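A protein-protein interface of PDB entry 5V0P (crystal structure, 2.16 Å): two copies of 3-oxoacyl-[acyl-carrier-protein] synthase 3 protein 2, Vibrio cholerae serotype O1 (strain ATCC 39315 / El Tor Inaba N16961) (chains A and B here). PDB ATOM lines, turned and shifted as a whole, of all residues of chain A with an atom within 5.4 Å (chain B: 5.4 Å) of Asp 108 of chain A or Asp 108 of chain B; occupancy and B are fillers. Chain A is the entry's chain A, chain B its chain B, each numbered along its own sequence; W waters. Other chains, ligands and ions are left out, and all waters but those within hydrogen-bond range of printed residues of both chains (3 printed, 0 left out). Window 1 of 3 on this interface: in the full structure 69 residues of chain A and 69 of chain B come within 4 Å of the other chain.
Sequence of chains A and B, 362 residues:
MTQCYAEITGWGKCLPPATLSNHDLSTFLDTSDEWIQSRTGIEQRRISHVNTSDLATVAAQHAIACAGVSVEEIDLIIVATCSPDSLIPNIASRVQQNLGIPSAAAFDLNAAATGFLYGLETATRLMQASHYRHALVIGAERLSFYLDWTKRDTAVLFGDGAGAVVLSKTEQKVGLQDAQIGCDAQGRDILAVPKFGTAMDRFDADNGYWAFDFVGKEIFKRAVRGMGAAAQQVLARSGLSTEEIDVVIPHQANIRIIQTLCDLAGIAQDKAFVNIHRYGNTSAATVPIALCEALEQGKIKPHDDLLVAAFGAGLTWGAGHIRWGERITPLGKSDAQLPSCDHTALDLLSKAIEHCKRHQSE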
ATOM      1  N   ILE A  78      30.962   1.869  25.283  1.00  0.00           N
ATOM      2  CA  ILE A  78      31.178   1.208  23.999  1.00  0.00           C
ATOM      3  C   ILE A  78      32.158   0.030  24.202  1.00  0.00           C
ATOM      4  O   ILE A  78      33.294   0.217  24.712  1.00  0.00           O
ATOM      5  CB  ILE A  78      31.778   2.167  22.938  1.00  0.00           C
ATOM      6  CG1 ILE A  78      30.898   3.405  22.766  1.00  0.00           C
ATOM      7  CG2 ILE A  78      31.991   1.420  21.628  1.00  0.00           C
ATOM      8  CD1 ILE A  78      31.401   4.421  21.777  1.00  0.00           C
ATOM      9  N   VAL A  79      31.738  -1.166  23.807  1.00  0.00           N
ATOM     10  CA  VAL A  79      32.634  -2.327  23.767  1.00  0.00           C
ATOM     11  C   VAL A  79      32.929  -2.623  22.296  1.00  0.00           C
ATOM     12  O   VAL A  79      32.049  -3.020  21.538  1.00  0.00           O
ATOM     13  CB  VAL A  79      32.025  -3.584  24.416  1.00  0.00           C
ATOM     14  CG1 VAL A  79      32.958  -4.798  24.241  1.00  0.00           C
ATOM     15  CG2 VAL A  79      31.728  -3.340  25.887  1.00  0.00           C
ATOM     16  N   THR A  81      34.365  -5.088  19.912  1.00  0.00           N
ATOM     17  CA  THR A  81      34.645  -6.536  19.894  1.00  0.00           C
ATOM     18  C   THR A  81      34.057  -7.195  18.653  1.00  0.00           C
ATOM     19  O   THR A  81      33.080  -6.707  18.094  1.00  0.00           O
ATOM     20  CB  THR A  81      34.065  -7.238  21.149  1.00  0.00           C
ATOM     21  OG1 THR A  81      34.445  -8.626  21.167  1.00  0.00           O
ATOM     22  CG2 THR A  81      32.571  -7.133  21.205  1.00  0.00           C
ATOM     23  N   PRO A  84      31.767 -11.246  20.829  1.00  0.00           N
ATOM     24  CA  PRO A  84      30.884 -11.054  21.978  1.00  0.00           C
ATOM     25  C   PRO A  84      30.240 -12.350  22.500  1.00  0.00           C
ATOM     26  O   PRO A  84      29.904 -13.236  21.706  1.00  0.00           O
ATOM     27  CB  PRO A  84      29.807 -10.129  21.415  1.00  0.00           C
ATOM     28  CG  PRO A  84      29.702 -10.543  19.985  1.00  0.00           C
ATOM     29  CD  PRO A  84      31.122 -10.806  19.573  1.00  0.00           C
ATOM     30  N   SER A  86      27.339 -12.839  23.540  1.00  0.00           N
ATOM     31  CA  SER A  86      26.002 -12.924  22.992  1.00  0.00           C
ATOM     32  C   SER A  86      25.784 -11.804  21.985  1.00  0.00           C
ATOM     33  O   SER A  86      26.466 -10.776  22.032  1.00  0.00           O
ATOM     34  CB  SER A  86      24.962 -12.804  24.115  1.00  0.00           C
ATOM     35  OG  SER A  86      25.156 -11.604  24.855  1.00  0.00           O
ATOM     36  N   ASN A  90      23.485  -7.118  23.721  1.00  0.00           N
ATOM     37  CA  ASN A  90      24.888  -6.764  23.518  1.00  0.00           C
ATOM     38  C   ASN A  90      25.668  -6.991  24.845  1.00  0.00           C
ATOM     39  O   ASN A  90      25.057  -7.188  25.908  1.00  0.00           O
ATOM     40  CB  ASN A  90      25.006  -5.327  22.963  1.00  0.00           C
ATOM     41  CG  ASN A  90      24.594  -4.246  23.958  1.00  0.00           C
ATOM     42  OD1 ASN A  90      24.757  -4.402  25.153  1.00  0.00           O
ATOM     43  ND2 ASN A  90      24.073  -3.139  23.455  1.00  0.00           N
ATOM     44  N   ILE A  91      26.993  -7.015  24.786  1.00  0.00           N
ATOM     45  CA  ILE A  91      27.792  -7.168  26.020  1.00  0.00           C
ATOM     46  C   ILE A  91      28.244  -5.873  26.682  1.00  0.00           C
ATOM     47  O   ILE A  91      28.684  -5.906  27.819  1.00  0.00           O
ATOM     48  CB  ILE A  91      28.996  -8.124  25.853  1.00  0.00           C
ATOM     49  CG1 ILE A  91      30.016  -7.600  24.847  1.00  0.00           C
ATOM     50  CG2 ILE A  91      28.509  -9.516  25.466  1.00  0.00           C
ATOM     51  CD1 ILE A  91      31.387  -8.231  25.045  1.00  0.00           C
ATOM     52  N   ALA A  92      28.140  -4.740  26.001  1.00  0.00           N
ATOM     53  CA  ALA A  92      28.253  -3.446  26.689  1.00  0.00           C
ATOM     54  C   ALA A  92      27.280  -3.388  27.873  1.00  0.00           C
ATOM     55  O   ALA A  92      27.641  -2.922  28.936  1.00  0.00           O
ATOM     56  CB  ALA A  92      27.983  -2.291  25.729  1.00  0.00           C
ATOM     57  N   SER A  93      26.048  -3.856  27.664  1.00  0.00           N
ATOM     58  CA  SER A  93      25.039  -3.938  28.733  1.00  0.00           C
ATOM     59  C   SER A  93      25.396  -4.911  29.865  1.00  0.00           C
ATOM     60  O   SER A  93      24.960  -4.715  31.005  1.00  0.00           O
ATOM     61  CB  SER A  93      23.657  -4.290  28.154  1.00  0.00           C
ATOM     62  OG  SER A  93      23.626  -5.600  27.601  1.00  0.00           O
ATOM     63  N   ALA A 106      24.709   2.134  25.947  1.00  0.00           N
ATOM     64  CA  ALA A 106      25.592   0.986  25.941  1.00  0.00           C
ATOM     65  C   ALA A 106      25.441   0.234  24.644  1.00  0.00           C
ATOM     66  O   ALA A 106      24.356  -0.304  24.374  1.00  0.00           O
ATOM     67  CB  ALA A 106      25.251   0.057  27.104  1.00  0.00           C
ATOM     68  N   PHE A 107      26.507   0.187  23.842  1.00  0.00           N
ATOM     69  CA  PHE A 107      26.470  -0.612  22.612  1.00  0.00           C
ATOM     70  C   PHE A 107      27.783  -1.311  22.263  1.00  0.00           C
ATOM     71  O   PHE A 107      28.874  -0.894  22.689  1.00  0.00           O
ATOM     72  CB  PHE A 107      25.921   0.229  21.439  1.00  0.00           C
ATOM     73  CG  PHE A 107      26.824   1.342  20.957  1.00  0.00           C
ATOM     74  CD1 PHE A 107      27.760   1.110  19.952  1.00  0.00           C
ATOM     75  CD2 PHE A 107      26.689   2.637  21.438  1.00  0.00           C
ATOM     76  CE1 PHE A 107      28.575   2.124  19.472  1.00  0.00           C
ATOM     77  CE2 PHE A 107      27.488   3.685  20.950  1.00  0.00           C
ATOM     78  CZ  PHE A 107      28.441   3.417  19.963  1.00  0.00           C
ATOM     79  N   ASP A 108      27.662  -2.391  21.496  1.00  0.00           N
ATOM     80  CA  ASP A 108      28.830  -3.047  20.919  1.00  0.00           C
ATOM     81  C   ASP A 108      29.082  -2.499  19.531  1.00  0.00           C
ATOM     82  O   ASP A 108      28.139  -2.236  18.776  1.00  0.00           O
ATOM     83  CB  ASP A 108      28.653  -4.568  20.866  1.00  0.00           C
ATOM     84  CG  ASP A 108      28.483  -5.180  22.250  1.00  0.00           C
ATOM     85  OD1 ASP A 108      28.601  -4.428  23.247  1.00  0.00           O
ATOM     86  OD2 ASP A 108      28.211  -6.411  22.363  1.00  0.00           O
ATOM     87  N   LEU A 109      30.363  -2.330  19.218  1.00  0.00           N
ATOM     88  CA  LEU A 109      30.823  -1.759  17.973  1.00  0.00           C
ATOM     89  C   LEU A 109      31.718  -2.812  17.364  1.00  0.00           C
ATOM     90  O   LEU A 109      32.656  -3.272  18.018  1.00  0.00           O
ATOM     91  CB  LEU A 109      31.598  -0.452  18.241  1.00  0.00           C
ATOM     92  CG  LEU A 109      31.932   0.396  17.013  1.00  0.00           C
ATOM     93  CD1 LEU A 109      32.155   1.871  17.373  1.00  0.00           C
ATOM     94  CD2 LEU A 109      33.124  -0.169  16.258  1.00  0.00           C
ATOM     95  N   ASN A 110      31.411  -3.226  16.130  1.00  0.00           N
ATOM     96  CA  ASN A 110      32.241  -4.184  15.425  1.00  0.00           C
ATOM     97  C   ASN A 110      32.882  -3.566  14.186  1.00  0.00           C
ATOM     98  O   ASN A 110      32.214  -3.408  13.145  1.00  0.00           O
ATOM     99  CB  ASN A 110      31.454  -5.442  15.052  1.00  0.00           C
ATOM    100  CG  ASN A 110      32.329  -6.511  14.417  1.00  0.00           C
ATOM    101  OD1 ASN A 110      33.558  -6.364  14.323  1.00  0.00           O
ATOM    102  ND2 ASN A 110      31.700  -7.602  13.975  1.00  0.00           N
ATOM    103  N   ALA A 111      34.189  -3.279  14.305  1.00  0.00           N
ATOM    104  CA  ALA A 111      35.059  -2.970  13.172  1.00  0.00           C
ATOM    105  C   ALA A 111      36.370  -3.769  13.263  1.00  0.00           C
ATOM    106  O   ALA A 111      37.429  -3.275  12.848  1.00  0.00           O
ATOM    107  CB  ALA A 111      35.350  -1.479  13.131  1.00  0.00           C
ATOM    108  N   ILE B  78      26.904   2.764   8.872  1.00  0.00           N
ATOM    109  CA  ILE B  78      26.569   2.067  10.116  1.00  0.00           C
ATOM    110  C   ILE B  78      25.401   1.091   9.846  1.00  0.00           C
ATOM    111  O   ILE B  78      24.322   1.499   9.353  1.00  0.00           O
ATOM    112  CB  ILE B  78      26.153   3.042  11.238  1.00  0.00           C
ATOM    113  CG1 ILE B  78      27.242   4.090  11.483  1.00  0.00           C
ATOM    114  CG2 ILE B  78      25.810   2.279  12.495  1.00  0.00           C
ATOM    115  CD1 ILE B  78      26.909   5.146  12.509  1.00  0.00           C
ATOM    116  N   VAL B  79      25.606  -0.184  10.155  1.00  0.00           N
ATOM    117  CA  VAL B  79      24.532  -1.172  10.126  1.00  0.00           C
ATOM    118  C   VAL B  79      24.178  -1.514  11.573  1.00  0.00           C
ATOM    119  O   VAL B  79      24.975  -2.116  12.293  1.00  0.00           O
ATOM    120  CB  VAL B  79      24.917  -2.475   9.386  1.00  0.00           C
ATOM    121  CG1 VAL B  79      23.794  -3.514   9.487  1.00  0.00           C
ATOM    122  CG2 VAL B  79      25.269  -2.179   7.938  1.00  0.00           C
ATOM    123  N   THR B  81      22.328  -3.862  13.779  1.00  0.00           N
ATOM    124  CA  THR B  81      21.803  -5.237  13.703  1.00  0.00           C
ATOM    125  C   THR B  81      22.270  -6.070  14.892  1.00  0.00           C
ATOM    126  O   THR B  81      23.315  -5.785  15.481  1.00  0.00           O
ATOM    127  CB  THR B  81      22.264  -5.938  12.403  1.00  0.00           C
ATOM    128  OG1 THR B  81      21.656  -7.242  12.291  1.00  0.00           O
ATOM    129  CG2 THR B  81      23.771  -6.092  12.355  1.00  0.00           C
ATOM    130  N   PRO B  84      23.855 -10.299  12.431  1.00  0.00           N
ATOM    131  CA  PRO B  84      24.766 -10.183  11.299  1.00  0.00           C
ATOM    132  C   PRO B  84      25.183 -11.519  10.680  1.00  0.00           C
ATOM    133  O   PRO B  84      25.355 -12.504  11.401  1.00  0.00           O
ATOM    134  CB  PRO B  84      25.982  -9.493  11.921  1.00  0.00           C
ATOM    135  CG  PRO B  84      26.005 -10.025  13.320  1.00  0.00           C
ATOM    136  CD  PRO B  84      24.555 -10.041  13.705  1.00  0.00           C
ATOM    137  N   SER B  86      27.963 -12.439   9.587  1.00  0.00           N
ATOM    138  CA  SER B  86      29.257 -12.791  10.129  1.00  0.00           C
ATOM    139  C   SER B  86      29.652 -11.798  11.207  1.00  0.00           C
ATOM    140  O   SER B  86      29.159 -10.661  11.224  1.00  0.00           O
ATOM    141  CB  SER B  86      30.304 -12.781   9.015  1.00  0.00           C
ATOM    142  OG  SER B  86      30.319 -11.527   8.342  1.00  0.00           O
ATOM    143  N   ASN B  90      32.730  -7.471   9.764  1.00  0.00           N
ATOM    144  CA  ASN B  90      31.408  -6.895  10.007  1.00  0.00           C
ATOM    145  C   ASN B  90      30.601  -6.889   8.677  1.00  0.00           C
ATOM    146  O   ASN B  90      31.169  -7.109   7.604  1.00  0.00           O
ATOM    147  CB  ASN B  90      31.536  -5.501  10.666  1.00  0.00           C
ATOM    148  CG  ASN B  90      32.128  -4.444   9.754  1.00  0.00           C
ATOM    149  OD1 ASN B  90      31.946  -4.480   8.550  1.00  0.00           O
ATOM    150  ND2 ASN B  90      32.831  -3.473  10.341  1.00  0.00           N
ATOM    151  N   ILE B  91      29.293  -6.681   8.745  1.00  0.00           N
ATOM    152  CA  ILE B  91      28.481  -6.611   7.513  1.00  0.00           C
ATOM    153  C   ILE B  91      28.261  -5.210   6.947  1.00  0.00           C
ATOM    154  O   ILE B  91      27.824  -5.083   5.813  1.00  0.00           O
ATOM    155  CB  ILE B  91      27.135  -7.349   7.622  1.00  0.00           C
ATOM    156  CG1 ILE B  91      26.219  -6.737   8.676  1.00  0.00           C
ATOM    157  CG2 ILE B  91      27.381  -8.829   7.908  1.00  0.00           C
ATOM    158  CD1 ILE B  91      24.761  -7.100   8.445  1.00  0.00           C
ATOM    159  N   ALA B  92      28.561  -4.159   7.704  1.00  0.00           N
ATOM    160  CA  ALA B  92      28.676  -2.828   7.106  1.00  0.00           C
ATOM    161  C   ALA B  92      29.654  -2.852   5.924  1.00  0.00           C
ATOM    162  O   ALA B  92      29.388  -2.260   4.896  1.00  0.00           O
ATOM    163  CB  ALA B  92      29.134  -1.806   8.137  1.00  0.00           C
ATOM    164  N   SER B  93      30.782  -3.538   6.094  1.00  0.00           N
ATOM    165  CA  SER B  93      31.772  -3.713   5.019  1.00  0.00           C
ATOM    166  C   SER B  93      31.255  -4.534   3.822  1.00  0.00           C
ATOM    167  O   SER B  93      31.725  -4.337   2.695  1.00  0.00           O
ATOM    168  CB  SER B  93      33.066  -4.343   5.563  1.00  0.00           C
ATOM    169  OG  SER B  93      32.866  -5.683   6.012  1.00  0.00           O
ATOM    170  N   ALA B 106      33.119   2.010   8.206  1.00  0.00           N
ATOM    171  CA  ALA B 106      32.041   1.029   8.137  1.00  0.00           C
ATOM    172  C   ALA B 106      32.057   0.167   9.371  1.00  0.00           C
ATOM    173  O   ALA B 106      33.021  -0.582   9.580  1.00  0.00           O
ATOM    174  CB  ALA B 106      32.206   0.153   6.897  1.00  0.00           C
ATOM    175  N   PHE B 107      31.003   0.244  10.175  1.00  0.00           N
ATOM    176  CA  PHE B 107      30.888  -0.630  11.350  1.00  0.00           C
ATOM    177  C   PHE B 107      29.475  -1.111  11.659  1.00  0.00           C
ATOM    178  O   PHE B 107      28.475  -0.490  11.262  1.00  0.00           O
ATOM    179  CB  PHE B 107      31.566   0.027  12.573  1.00  0.00           C
ATOM    180  CG  PHE B 107      30.861   1.245  13.131  1.00  0.00           C
ATOM    181  CD1 PHE B 107      29.893   1.111  14.122  1.00  0.00           C
ATOM    182  CD2 PHE B 107      31.225   2.525  12.740  1.00  0.00           C
ATOM    183  CE1 PHE B 107      29.268   2.237  14.677  1.00  0.00           C
ATOM    184  CE2 PHE B 107      30.617   3.660  13.301  1.00  0.00           C
ATOM    185  CZ  PHE B 107      29.631   3.508  14.265  1.00  0.00           C
ATOM    186  N   ASP B 108      29.405  -2.242  12.360  1.00  0.00           N
ATOM    187  CA  ASP B 108      28.141  -2.731  12.893  1.00  0.00           C
ATOM    188  C   ASP B 108      27.978  -2.239  14.311  1.00  0.00           C
ATOM    189  O   ASP B 108      28.943  -2.212  15.079  1.00  0.00           O
ATOM    190  CB  ASP B 108      28.064  -4.259  12.840  1.00  0.00           C
ATOM    191  CG  ASP B 108      28.136  -4.796  11.415  1.00  0.00           C
ATOM    192  OD1 ASP B 108      28.149  -3.969  10.473  1.00  0.00           O
ATOM    193  OD2 ASP B 108      28.195  -6.050  11.221  1.00  0.00           O
ATOM    194  N   LEU B 109      26.742  -1.869  14.644  1.00  0.00           N
ATOM    195  CA  LEU B 109      26.382  -1.315  15.923  1.00  0.00           C
ATOM    196  C   LEU B 109      25.311  -2.233  16.468  1.00  0.00           C
ATOM    197  O   LEU B 109      24.304  -2.476  15.793  1.00  0.00           O
ATOM    198  CB  LEU B 109      25.854   0.127  15.749  1.00  0.00           C
ATOM    199  CG  LEU B 109      25.662   0.934  17.034  1.00  0.00           C
ATOM    200  CD1 LEU B 109      25.677   2.434  16.759  1.00  0.00           C
ATOM    201  CD2 LEU B 109      24.383   0.536  17.761  1.00  0.00           C
ATOM    202  N   ASN B 110      25.533  -2.768  17.668  1.00  0.00           N
ATOM    203  CA  ASN B 110      24.544  -3.608  18.317  1.00  0.00           C
ATOM    204  C   ASN B 110      24.015  -2.978  19.598  1.00  0.00           C
ATOM    205  O   ASN B 110      24.694  -2.994  20.631  1.00  0.00           O
ATOM    206  CB  ASN B 110      25.103  -5.010  18.595  1.00  0.00           C
ATOM    207  CG  ASN B 110      24.068  -5.948  19.165  1.00  0.00           C
ATOM    208  OD1 ASN B 110      22.871  -5.605  19.277  1.00  0.00           O
ATOM    209  ND2 ASN B 110      24.510  -7.143  19.527  1.00  0.00           N
ATOM    210  N   ALA B 111      22.784  -2.465  19.515  1.00  0.00           N
ATOM    211  CA  ALA B 111      21.969  -2.083  20.667  1.00  0.00           C
ATOM    212  C   ALA B 111      20.544  -2.632  20.531  1.00  0.00           C
ATOM    213  O   ALA B 111      19.585  -1.987  20.978  1.00  0.00           O
ATOM    214  CB  ALA B 111      21.943  -0.561  20.807  1.00  0.00           C
HETATM  215  O   HOH W   1      28.284  -4.761  16.857  1.00  0.00           O
HETATM  216  O   HOH W   2      28.972  -8.160  12.827  1.00  0.00           O
HETATM  217  O   HOH W   3      27.109  -8.160  20.539  1.00  0.00           O
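Among the printed residues, merely in contact across the chains: Asn 90 of chain A with Ala 111 of chain B, Phe 107 of chain A with Leu 109 of chain B, Phe 107 of chain A with Asn 110 of chain B, Asp 108 of chain A with Asp 108 of chain B, Asp 108 of chain A with Leu 109 of chain B, Leu 109 of chain A with Phe 107 of chain B, Leu 109 of chain A with Asp 108 of chain B, Asn 110 of chain A with Phe 107 of chain B and Ala 111 of chain A with Asn 90 of chain B.
Asn 90 of chain A touches Asn 110 of chain B, and with the chains exchanged Asn 110 of chain A touches Asn 90 of chain B.
Asn 90 of chain A touches Ala 111 of chain B, and with the chains exchanged Ala 111 of chain A touches Asn 90 of chain B.
Phe 107 of chain A touches Leu 109 of chain B, and with the chains exchanged Leu 109 of chain A touches Phe 107 of chain B.
Phe 107 of chain A touches Asn 110 of chain B, and with the chains exchanged Asn 110 of chain A touches Phe 107 of chain B.
Positions printed for both chains: 78, 79, 81, 84, 86, 90, 91, 92, 93, 106, 107, 108, 109, 110 and 111.
Of the 13 pairs that touch across the chains among the printed residues, 13 have their exchanged pair printed and touching as well.
Asp 108 of chain A touches three residues of chain B.
Asp 108 of chain B touches just these residues of chain A: Asp 108 (3.8 Å), Leu 109 (3.5 Å) and Asn 110 (2.9 Å).
Of the printed residues of chain A, Asn 110 of chain B touches Asn 90 (2.9 Å), Phe 107 (3.5 Å) and Asp 108 (2.9 Å).
Printed residues of chain B within 4 Å of Asn 90 of chain A: Asn 110 (2.9 Å) and Ala 111 (3.6 Å).
Ser 86 of chain A touches none of the printed residues of chain B.
Ala 92 of chain B touches none of the printed residues of chain A.
Water W3 lies within hydrogen-bond range of OD2 of Asp 108 of chain A (2.8 Å), ND2 of Asn 110 of chain B (3.0 Å) and O of Ser 86 of chain A (3.1 Å).
Water W2 lies within hydrogen-bond range of the side-chain carboxylate of Asp 108 of chain B (2.8 Å), the backbone carbonyl oxygen of Ser 86 of chain B (3.0 Å) and the side-chain amide nitrogen of Asn 110 of chain A (3.0 Å).
Water W1 lies within hydrogen-bond range of the backbone carbonyl oxygen (O) of Asp 108 of chain A (3.2 Å), the backbone carbonyl oxygen (O) of Asp 108 of chain B (3.2 Å) and the backbone NH (N) of Asn 110 of chain B (3.5 Å).
O of Asn 110 of chain B lies within hydrogen-bond range of ND2 of Asn 90 of chain A, at 2.9 Å.
N of Asn 110 of chain A is in hydrogen-bond range of O of Asp 108 of chain B (2.9 Å).
The backbone carbonyl oxygen (O) of Asp 108 of chain A lies within hydrogen-bond range of the backbone NH (N) of Asn 110 of chain B (2.9 Å).
The side-chain amide nitrogen (ND2) of Asn 90 of chain B sits at hydrogen-bond distance from the backbone carbonyl oxygen (O) of Asn 110 of chain A, 2.9 Å away.
Hydrophobic or aromatic side chains of chain A that line the printed part of chain B: Phe 107 and Leu 109.
Along chain A the printed residues that touch a printed residue of chain B span positions 90 to 111.
Of the 15 printed residues of chain B, 6 touch a printed residue of chain A.
Hydrophobic or aromatic side chains of chain B within 4 Å of the printed part of chain A: Phe 107 and Leu 109.
Among the printed residues, 13 pairs touch across the chains.
Among the printed residues, no Asp or Glu carboxylate lies within 4 Å of a Lys or Arg side-chain nitrogen of the other chain.
The side-chain carboxylate of Asp 108 of chain A sits at hydrogen-bond distance from the backbone NH of Ile 91 of chain A.
OD1 of Asp 108 of chain A sits at hydrogen-bond distance from N of Ala 92 of chain A, at 2.8 Å.
The side-chain amide nitrogen (ND2) of Asn 90 of chain B sits at hydrogen-bond distance from the backbone carbonyl oxygen (O) of Ala 106 of chain B (3.0 Å).
The backbone NH (N) of Leu 109 of chain B lies within hydrogen-bond range of the backbone carbonyl oxygen (O) of Val 79 of chain B (3.0 Å).
N of Thr 81 of chain A is in hydrogen-bond range of O of Leu 109 of chain A (3.1 Å).
O of Asn 90 of chain B sits at hydrogen-bond distance from OG of Ser 93 of chain B, at 2.7 Å.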
